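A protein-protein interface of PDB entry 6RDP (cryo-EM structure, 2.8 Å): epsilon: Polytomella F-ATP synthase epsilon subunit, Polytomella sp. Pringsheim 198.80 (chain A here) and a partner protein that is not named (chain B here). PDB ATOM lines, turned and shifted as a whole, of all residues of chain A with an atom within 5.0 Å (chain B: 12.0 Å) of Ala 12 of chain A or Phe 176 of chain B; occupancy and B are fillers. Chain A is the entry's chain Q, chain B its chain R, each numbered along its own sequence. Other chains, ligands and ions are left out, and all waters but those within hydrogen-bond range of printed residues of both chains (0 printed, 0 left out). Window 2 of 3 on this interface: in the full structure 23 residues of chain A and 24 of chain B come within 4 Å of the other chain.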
ATOM      1  N   PHE A   8      -1.583  22.880 -13.485  1.00  0.00           N
ATOM      2  CA  PHE A   8      -2.521  21.938 -14.085  1.00  0.00           C
ATOM      3  C   PHE A   8      -3.874  22.568 -14.365  1.00  0.00           C
ATOM      4  O   PHE A   8      -4.607  22.087 -15.234  1.00  0.00           O
ATOM      5  CB  PHE A   8      -2.682  20.710 -13.194  1.00  0.00           C
ATOM      6  CG  PHE A   8      -3.413  20.966 -11.908  1.00  0.00           C
ATOM      7  CD1 PHE A   8      -4.737  20.595 -11.766  1.00  0.00           C
ATOM      8  CD2 PHE A   8      -2.762  21.531 -10.824  1.00  0.00           C
ATOM      9  CE1 PHE A   8      -5.406  20.813 -10.581  1.00  0.00           C
ATOM     10  CE2 PHE A   8      -3.425  21.753  -9.637  1.00  0.00           C
ATOM     11  CZ  PHE A   8      -4.749  21.390  -9.517  1.00  0.00           C
ATOM     12  N   TYR A   9      -4.229  23.630 -13.647  1.00  0.00           N
ATOM     13  CA  TYR A   9      -5.433  24.369 -14.002  1.00  0.00           C
ATOM     14  C   TYR A   9      -5.183  25.296 -15.183  1.00  0.00           C
ATOM     15  O   TYR A   9      -6.062  25.470 -16.029  1.00  0.00           O
ATOM     16  CB  TYR A   9      -5.950  25.155 -12.793  1.00  0.00           C
ATOM     17  CG  TYR A   9      -4.903  25.945 -12.037  1.00  0.00           C
ATOM     18  CD1 TYR A   9      -4.280  25.414 -10.921  1.00  0.00           C
ATOM     19  CD2 TYR A   9      -4.565  27.233 -12.422  1.00  0.00           C
ATOM     20  CE1 TYR A   9      -3.338  26.132 -10.228  1.00  0.00           C
ATOM     21  CE2 TYR A   9      -3.620  27.956 -11.739  1.00  0.00           C
ATOM     22  CZ  TYR A   9      -3.010  27.405 -10.645  1.00  0.00           C
ATOM     23  OH  TYR A   9      -2.070  28.135  -9.961  1.00  0.00           O
ATOM     24  N   ARG A  10      -3.985  25.865 -15.274  1.00  0.00           N
ATOM     25  CA  ARG A  10      -3.703  26.886 -16.272  1.00  0.00           C
ATOM     26  C   ARG A  10      -3.546  26.300 -17.668  1.00  0.00           C
ATOM     27  O   ARG A  10      -3.951  26.933 -18.651  1.00  0.00           O
ATOM     28  CB  ARG A  10      -2.445  27.655 -15.875  1.00  0.00           C
ATOM     29  CG  ARG A  10      -2.125  28.823 -16.766  1.00  0.00           C
ATOM     30  CD  ARG A  10      -3.244  29.830 -16.717  1.00  0.00           C
ATOM     31  NE  ARG A  10      -3.470  30.298 -15.358  1.00  0.00           N
ATOM     32  CZ  ARG A  10      -4.030  31.462 -15.064  1.00  0.00           C
ATOM     33  NH1 ARG A  10      -4.418  32.265 -16.041  1.00  0.00           N
ATOM     34  NH2 ARG A  10      -4.191  31.824 -13.804  1.00  0.00           N
ATOM     35  N   VAL A  11      -2.984  25.094 -17.777  1.00  0.00           N
ATOM     36  CA  VAL A  11      -2.822  24.463 -19.081  1.00  0.00           C
ATOM     37  C   VAL A  11      -4.152  23.968 -19.629  1.00  0.00           C
ATOM     38  O   VAL A  11      -4.294  23.801 -20.844  1.00  0.00           O
ATOM     39  CB  VAL A  11      -1.804  23.311 -19.000  1.00  0.00           C
ATOM     40  CG1 VAL A  11      -0.421  23.848 -18.698  1.00  0.00           C
ATOM     41  CG2 VAL A  11      -2.218  22.294 -17.950  1.00  0.00           C
ATOM     42  N   ALA A  12      -5.143  23.753 -18.767  1.00  0.00           N
ATOM     43  CA  ALA A  12      -6.450  23.267 -19.176  1.00  0.00           C
ATOM     44  C   ALA A  12      -7.393  24.385 -19.599  1.00  0.00           C
ATOM     45  O   ALA A  12      -8.596  24.141 -19.731  1.00  0.00           O
ATOM     46  CB  ALA A  12      -7.084  22.457 -18.045  1.00  0.00           C
ATOM     47  N   GLY A  13      -6.879  25.600 -19.807  1.00  0.00           N
ATOM     48  CA  GLY A  13      -7.696  26.747 -20.147  1.00  0.00           C
ATOM     49  C   GLY A  13      -8.351  27.447 -18.975  1.00  0.00           C
ATOM     50  O   GLY A  13      -8.865  28.559 -19.148  1.00  0.00           O
ATOM     51  N   MET A  14      -8.346  26.840 -17.793  1.00  0.00           N
ATOM     52  CA  MET A  14      -9.008  27.410 -16.630  1.00  0.00           C
ATOM     53  C   MET A  14      -8.188  28.556 -16.054  1.00  0.00           C
ATOM     54  O   MET A  14      -6.955  28.535 -16.085  1.00  0.00           O
ATOM     55  CB  MET A  14      -9.210  26.324 -15.575  1.00  0.00           C
ATOM     56  CG  MET A  14     -10.135  26.686 -14.445  1.00  0.00           C
ATOM     57  SD  MET A  14     -10.080  25.462 -13.133  1.00  0.00           S
ATOM     58  CE  MET A  14     -10.360  23.966 -14.055  1.00  0.00           C
ATOM     59  N   ARG A  18     -11.091  30.443 -10.839  1.00  0.00           N
ATOM     60  CA  ARG A  18     -12.063  29.364 -10.922  1.00  0.00           C
ATOM     61  C   ARG A  18     -11.576  28.125 -10.191  1.00  0.00           C
ATOM     62  O   ARG A  18     -12.360  27.457  -9.517  1.00  0.00           O
ATOM     63  CB  ARG A  18     -12.361  29.030 -12.374  1.00  0.00           C
ATOM     64  CG  ARG A  18     -13.659  28.286 -12.535  1.00  0.00           C
ATOM     65  CD  ARG A  18     -14.008  28.131 -13.990  1.00  0.00           C
ATOM     66  NE  ARG A  18     -14.654  29.305 -14.551  1.00  0.00           N
ATOM     67  CZ  ARG A  18     -15.967  29.476 -14.578  1.00  0.00           C
ATOM     68  NH1 ARG A  18     -16.766  28.550 -14.069  1.00  0.00           N
ATOM     69  NH2 ARG A  18     -16.479  30.571 -15.114  1.00  0.00           N
ATOM     70  N   PRO A  70     -19.604  27.307 -11.475  1.00  0.00           N
ATOM     71  CA  PRO A  70     -19.805  26.114 -12.316  1.00  0.00           C
ATOM     72  C   PRO A  70     -18.525  25.297 -12.420  1.00  0.00           C
ATOM     73  O   PRO A  70     -17.487  25.801 -12.852  1.00  0.00           O
ATOM     74  CB  PRO A  70     -20.214  26.690 -13.678  1.00  0.00           C
ATOM     75  CG  PRO A  70     -20.552  28.091 -13.445  1.00  0.00           C
ATOM     76  CD  PRO A  70     -19.830  28.548 -12.237  1.00  0.00           C
ATOM     77  N   LYS A  71     -18.611  24.021 -12.025  1.00  0.00           N
ATOM     78  CA  LYS A  71     -17.492  23.099 -12.200  1.00  0.00           C
ATOM     79  C   LYS A  71     -17.250  22.760 -13.663  1.00  0.00           C
ATOM     80  O   LYS A  71     -16.131  22.378 -14.022  1.00  0.00           O
ATOM     81  CB  LYS A  71     -17.738  21.815 -11.408  1.00  0.00           C
ATOM     82  CG  LYS A  71     -17.897  22.029  -9.920  1.00  0.00           C
ATOM     83  CD  LYS A  71     -18.112  20.715  -9.202  1.00  0.00           C
ATOM     84  CE  LYS A  71     -18.005  20.882  -7.695  1.00  0.00           C
ATOM     85  NZ  LYS A  71     -19.063  21.764  -7.130  1.00  0.00           N
ATOM     86  N   THR A  72     -18.263  22.914 -14.511  1.00  0.00           N
ATOM     87  CA  THR A  72     -18.160  22.621 -15.930  1.00  0.00           C
ATOM     88  C   THR A  72     -17.356  23.743 -16.606  1.00  0.00           C
ATOM     89  O   THR A  72     -17.021  24.756 -15.987  1.00  0.00           O
ATOM     90  CB  THR A  72     -19.574  22.454 -16.492  1.00  0.00           C
ATOM     91  OG1 THR A  72     -20.359  21.754 -15.521  1.00  0.00           O
ATOM     92  CG2 THR A  72     -19.600  21.579 -17.749  1.00  0.00           C
ATOM     93  N   ALA A  73     -17.034  23.559 -17.887  1.00  0.00           N
ATOM     94  CA  ALA A  73     -16.179  24.487 -18.615  1.00  0.00           C
ATOM     95  C   ALA A  73     -16.846  25.844 -18.801  1.00  0.00           C
ATOM     96  O   ALA A  73     -18.061  25.948 -18.992  1.00  0.00           O
ATOM     97  CB  ALA A  73     -15.804  23.913 -19.978  1.00  0.00           C
ATOM     98  N   ASN A  74     -16.028  26.889 -18.725  1.00  0.00           N
ATOM     99  CA  ASN A  74     -16.494  28.265 -18.824  1.00  0.00           C
ATOM    100  C   ASN A  74     -16.844  28.639 -20.262  1.00  0.00           C
ATOM    101  O   ASN A  74     -17.999  28.532 -20.677  1.00  0.00           O
ATOM    102  CB  ASN A  74     -15.429  29.213 -18.270  1.00  0.00           C
ATOM    103  CG  ASN A  74     -15.864  30.659 -18.286  1.00  0.00           C
ATOM    104  OD1 ASN A  74     -17.036  30.973 -18.072  1.00  0.00           O
ATOM    105  ND2 ASN A  74     -14.914  31.558 -18.522  1.00  0.00           N
ATOM    106  N   ALA B 167     -15.515  11.066  -6.516  1.00  0.00           N
ATOM    107  CA  ALA B 167     -14.479  11.823  -7.206  1.00  0.00           C
ATOM    108  C   ALA B 167     -13.433  10.924  -7.847  1.00  0.00           C
ATOM    109  O   ALA B 167     -12.716  11.372  -8.746  1.00  0.00           O
ATOM    110  CB  ALA B 167     -13.796  12.786  -6.238  1.00  0.00           C
ATOM    111  N   ALA B 170     -15.921   9.585 -11.634  1.00  0.00           N
ATOM    112  CA  ALA B 170     -16.160  10.403 -12.818  1.00  0.00           C
ATOM    113  C   ALA B 170     -14.814  10.882 -13.337  1.00  0.00           C
ATOM    114  O   ALA B 170     -14.327  11.946 -12.949  1.00  0.00           O
ATOM    115  CB  ALA B 170     -17.079  11.572 -12.490  1.00  0.00           C
ATOM    116  N   GLN B 171     -14.201  10.090 -14.217  1.00  0.00           N
ATOM    117  CA  GLN B 171     -12.900  10.405 -14.804  1.00  0.00           C
ATOM    118  C   GLN B 171     -13.082  10.551 -16.308  1.00  0.00           C
ATOM    119  O   GLN B 171     -12.901   9.581 -17.060  1.00  0.00           O
ATOM    120  CB  GLN B 171     -11.871   9.327 -14.479  1.00  0.00           C
ATOM    121  CG  GLN B 171     -11.643   9.124 -12.995  1.00  0.00           C
ATOM    122  CD  GLN B 171     -11.228  10.396 -12.285  1.00  0.00           C
ATOM    123  OE1 GLN B 171     -11.992  10.947 -11.500  1.00  0.00           O
ATOM    124  NE2 GLN B 171     -10.018  10.874 -12.563  1.00  0.00           N
ATOM    125  N   PRO B 172     -13.436  11.736 -16.792  1.00  0.00           N
ATOM    126  CA  PRO B 172     -13.625  11.928 -18.229  1.00  0.00           C
ATOM    127  C   PRO B 172     -12.342  12.395 -18.906  1.00  0.00           C
ATOM    128  O   PRO B 172     -11.342  12.715 -18.261  1.00  0.00           O
ATOM    129  CB  PRO B 172     -14.703  13.024 -18.296  1.00  0.00           C
ATOM    130  CG  PRO B 172     -14.863  13.543 -16.873  1.00  0.00           C
ATOM    131  CD  PRO B 172     -13.763  12.959 -16.049  1.00  0.00           C
ATOM    132  N   THR B 173     -12.398  12.436 -20.233  1.00  0.00           N
ATOM    133  CA  THR B 173     -11.323  13.004 -21.029  1.00  0.00           C
ATOM    134  C   THR B 173     -11.344  14.526 -21.028  1.00  0.00           C
ATOM    135  O   THR B 173     -10.375  15.143 -21.487  1.00  0.00           O
ATOM    136  CB  THR B 173     -11.396  12.494 -22.472  1.00  0.00           C
ATOM    137  OG1 THR B 173     -12.481  13.131 -23.155  1.00  0.00           O
ATOM    138  CG2 THR B 173     -11.605  10.989 -22.490  1.00  0.00           C
ATOM    139  N   ASP B 174     -12.419  15.139 -20.531  1.00  0.00           N
ATOM    140  CA  ASP B 174     -12.504  16.591 -20.448  1.00  0.00           C
ATOM    141  C   ASP B 174     -11.523  17.102 -19.405  1.00  0.00           C
ATOM    142  O   ASP B 174     -11.777  16.993 -18.201  1.00  0.00           O
ATOM    143  CB  ASP B 174     -13.925  17.017 -20.096  1.00  0.00           C
ATOM    144  CG  ASP B 174     -14.139  18.505 -20.260  1.00  0.00           C
ATOM    145  OD1 ASP B 174     -15.009  19.062 -19.561  1.00  0.00           O
ATOM    146  OD2 ASP B 174     -13.431  19.116 -21.087  1.00  0.00           O
ATOM    147  N   GLU B 175     -10.412  17.683 -19.872  1.00  0.00           N
ATOM    148  CA  GLU B 175      -9.341  18.089 -18.968  1.00  0.00           C
ATOM    149  C   GLU B 175      -9.731  19.280 -18.107  1.00  0.00           C
ATOM    150  O   GLU B 175      -9.070  19.551 -17.103  1.00  0.00           O
ATOM    151  CB  GLU B 175      -8.062  18.392 -19.747  1.00  0.00           C
ATOM    152  CG  GLU B 175      -7.390  17.150 -20.300  1.00  0.00           C
ATOM    153  CD  GLU B 175      -6.849  16.243 -19.203  1.00  0.00           C
ATOM    154  OE1 GLU B 175      -6.395  16.765 -18.164  1.00  0.00           O
ATOM    155  OE2 GLU B 175      -6.892  15.005 -19.373  1.00  0.00           O
ATOM    156  N   PHE B 176     -10.785  20.005 -18.478  1.00  0.00           N
ATOM    157  CA  PHE B 176     -11.382  20.932 -17.527  1.00  0.00           C
ATOM    158  C   PHE B 176     -11.994  20.167 -16.360  1.00  0.00           C
ATOM    159  O   PHE B 176     -11.659  20.408 -15.193  1.00  0.00           O
ATOM    160  CB  PHE B 176     -12.438  21.793 -18.218  1.00  0.00           C
ATOM    161  CG  PHE B 176     -12.718  23.075 -17.505  1.00  0.00           C
ATOM    162  CD1 PHE B 176     -12.042  24.230 -17.856  1.00  0.00           C
ATOM    163  CD2 PHE B 176     -13.615  23.120 -16.453  1.00  0.00           C
ATOM    164  CE1 PHE B 176     -12.283  25.413 -17.195  1.00  0.00           C
ATOM    165  CE2 PHE B 176     -13.852  24.297 -15.781  1.00  0.00           C
ATOM    166  CZ  PHE B 176     -13.185  25.443 -16.156  1.00  0.00           C
ATOM    167  N   GLU B 177     -12.881  19.220 -16.666  1.00  0.00           N
ATOM    168  CA  GLU B 177     -13.477  18.394 -15.625  1.00  0.00           C
ATOM    169  C   GLU B 177     -12.446  17.462 -15.004  1.00  0.00           C
ATOM    170  O   GLU B 177     -12.523  17.158 -13.812  1.00  0.00           O
ATOM    171  CB  GLU B 177     -14.658  17.608 -16.200  1.00  0.00           C
ATOM    172  CG  GLU B 177     -15.459  16.788 -15.185  1.00  0.00           C
ATOM    173  CD  GLU B 177     -15.812  17.567 -13.935  1.00  0.00           C
ATOM    174  OE1 GLU B 177     -16.665  18.472 -14.019  1.00  0.00           O
ATOM    175  OE2 GLU B 177     -15.243  17.265 -12.866  1.00  0.00           O
ATOM    176  N   GLN B 178     -11.442  17.037 -15.773  1.00  0.00           N
ATOM    177  CA  GLN B 178     -10.418  16.178 -15.187  1.00  0.00           C
ATOM    178  C   GLN B 178      -9.489  16.964 -14.268  1.00  0.00           C
ATOM    179  O   GLN B 178      -9.037  16.434 -13.249  1.00  0.00           O
ATOM    180  CB  GLN B 178      -9.620  15.471 -16.280  1.00  0.00           C
ATOM    181  CG  GLN B 178      -8.696  14.389 -15.755  1.00  0.00           C
ATOM    182  CD  GLN B 178      -9.454  13.315 -14.998  1.00  0.00           C
ATOM    183  OE1 GLN B 178      -9.415  13.261 -13.771  1.00  0.00           O
ATOM    184  NE2 GLN B 178     -10.159  12.460 -15.729  1.00  0.00           N
ATOM    185  N   ALA B 179      -9.222  18.232 -14.588  1.00  0.00           N
ATOM    186  CA  ALA B 179      -8.438  19.079 -13.699  1.00  0.00           C
ATOM    187  C   ALA B 179      -9.227  19.422 -12.443  1.00  0.00           C
ATOM    188  O   ALA B 179      -8.658  19.499 -11.344  1.00  0.00           O
ATOM    189  CB  ALA B 179      -8.007  20.348 -14.432  1.00  0.00           C
ATOM    190  N   ALA B 180     -10.542  19.611 -12.587  1.00  0.00           N
ATOM    191  CA  ALA B 180     -11.399  19.773 -11.418  1.00  0.00           C
ATOM    192  C   ALA B 180     -11.435  18.508 -10.573  1.00  0.00           C
ATOM    193  O   ALA B 180     -11.449  18.591  -9.343  1.00  0.00           O
ATOM    194  CB  ALA B 180     -12.808  20.169 -11.849  1.00  0.00           C
ATOM    195  N   ASN B 181     -11.412  17.334 -11.212  1.00  0.00           N
ATOM    196  CA  ASN B 181     -11.323  16.075 -10.482  1.00  0.00           C
ATOM    197  C   ASN B 181      -9.983  15.916  -9.786  1.00  0.00           C
ATOM    198  O   ASN B 181      -9.929  15.361  -8.685  1.00  0.00           O
ATOM    199  CB  ASN B 181     -11.556  14.898 -11.425  1.00  0.00           C
ATOM    200  CG  ASN B 181     -13.019  14.557 -11.584  1.00  0.00           C
ATOM    201  OD1 ASN B 181     -13.606  14.757 -12.647  1.00  0.00           O
ATOM    202  ND2 ASN B 181     -13.615  14.013 -10.531  1.00  0.00           N
ATOM    203  N   ARG B 182      -8.900  16.382 -10.413  1.00  0.00           N
ATOM    204  CA  ARG B 182      -7.582  16.329  -9.791  1.00  0.00           C
ATOM    205  C   ARG B 182      -7.526  17.210  -8.553  1.00  0.00           C
ATOM    206  O   ARG B 182      -7.044  16.776  -7.496  1.00  0.00           O
ATOM    207  CB  ARG B 182      -6.514  16.755 -10.801  1.00  0.00           C
ATOM    208  CG  ARG B 182      -5.117  16.910 -10.223  1.00  0.00           C
ATOM    209  CD  ARG B 182      -4.087  17.023 -11.329  1.00  0.00           C
ATOM    210  NE  ARG B 182      -2.800  17.505 -10.840  1.00  0.00           N
ATOM    211  CZ  ARG B 182      -1.728  17.679 -11.608  1.00  0.00           C
ATOM    212  NH1 ARG B 182      -1.787  17.413 -12.906  1.00  0.00           N
ATOM    213  NH2 ARG B 182      -0.597  18.124 -11.078  1.00  0.00           N
ATOM    214  N   ALA B 183      -8.045  18.437  -8.666  1.00  0.00           N
ATOM    215  CA  ALA B 183      -8.136  19.326  -7.512  1.00  0.00           C
ATOM    216  C   ALA B 183      -9.051  18.748  -6.439  1.00  0.00           C
ATOM    217  O   ALA B 183      -8.766  18.870  -5.241  1.00  0.00           O
ATOM    218  CB  ALA B 183      -8.631  20.701  -7.955  1.00  0.00           C
ATOM    219  N   ALA B 184     -10.121  18.066  -6.860  1.00  0.00           N
ATOM    220  CA  ALA B 184     -11.057  17.450  -5.930  1.00  0.00           C
ATOM    221  C   ALA B 184     -10.410  16.325  -5.139  1.00  0.00           C
ATOM    222  O   ALA B 184     -10.505  16.300  -3.906  1.00  0.00           O
ATOM    223  CB  ALA B 184     -12.270  16.923  -6.694  1.00  0.00           C
ATOM    224  N   ILE B 185      -9.733  15.400  -5.825  1.00  0.00           N
ATOM    225  CA  ILE B 185      -9.132  14.264  -5.137  1.00  0.00           C
ATOM    226  C   ILE B 185      -7.944  14.713  -4.302  1.00  0.00           C
ATOM    227  O   ILE B 185      -7.690  14.155  -3.232  1.00  0.00           O
ATOM    228  CB  ILE B 185      -8.750  13.140  -6.125  1.00  0.00           C
ATOM    229  CG1 ILE B 185      -7.688  13.585  -7.132  1.00  0.00           C
ATOM    230  CG2 ILE B 185      -9.979  12.624  -6.856  1.00  0.00           C
ATOM    231  CD1 ILE B 185      -7.125  12.451  -7.967  1.00  0.00           C
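The guanidinium group of Arg 18 of chain A sits at hydrogen-bond distance from the backbone carbonyl oxygen of Pro 70 of chain A (3.1 Å). O of Glu 177 of chain B lies close to OD1 of Asn 181 of chain B (2.9 Å). The guanidinium group of Arg 18 of chain A sits at hydrogen-bond distance from the side-chain amide oxygen of Asn 74 of chain A, at 3.0 Å. The backbone NH (N) of Met 14 of chain A lies within hydrogen-bond range of the backbone carbonyl oxygen (O) of Tyr 9 of chain A (3.2 Å).
Among the printed residues, pairs that only touch across the chains: Thr 72 of chain A with Phe 176 of chain B (3.2 Å), Phe 8 of chain A with Arg 182 of chain B (3.4 Å), Lys 71 of chain A with Phe 176 of chain B (3.5 Å), Arg 18 of chain A with Phe 176 of chain B (3.5 Å), Phe 8 of chain A with Ala 179 of chain B (3.6 Å), Met 14 of chain A with Phe 176 of chain B (3.6 Å), Ala 73 of chain A with Phe 176 of chain B (3.6 Å), Ala 12 of chain A with Glu 175 of chain B (3.6 Å), Ala 12 of chain A with Phe 176 of chain B (3.9 Å) and Lys 71 of chain A with Glu 177 of chain B (3.9 Å).
Hydrophobic or aromatic side chains of chain B within 4 Å of the printed part of chain A: Phe 176 and Ala 179. Among the printed residues, no Asp or Glu carboxylate lies within 4 Å of a Lys or Arg side-chain nitrogen of the other chain.
Of the printed residues of chain B, Phe 8 of chain A touches Ala 179 (3.6 Å) and Arg 182 (3.4 Å). Of the printed residues of chain B, Ala 12 of chain A touches Glu 175 and Phe 176. Met 14 of chain A touches one residue of chain B. Printed residues of chain B within 4 Å of Lys 71 of chain A: Phe 176 (3.5 Å) and Glu 177 (3.9 Å). Of chain B, only Phe 176 (3.2 Å) comes within 4 Å of Thr 72 of chain A. No residue of chain B comes within 4 Å of Asn 74 of chain A. Thr 173 of chain B touches none of the printed residues of chain A. Of the printed residues of chain A, Glu 175 of chain B touches Ala 12 (3.6 Å). Of chain A, only Ala 12, Met 14, Arg 18, Lys 71, Thr 72 and Ala 73 come within 4 Å of Phe 176 of chain B. Of the printed residues of chain A, Ala 179 of chain B touches Phe 8. Ala 183 of chain B touches none of the printed residues of chain A. The nearest residue of chain B that does not touch Ala 12 of chain A is Ala 179 of chain B (4.3 Å). The nearest printed residue of chain A that does not touch Arg 182 of chain B is Tyr 9 of chain A (6.7 Å).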
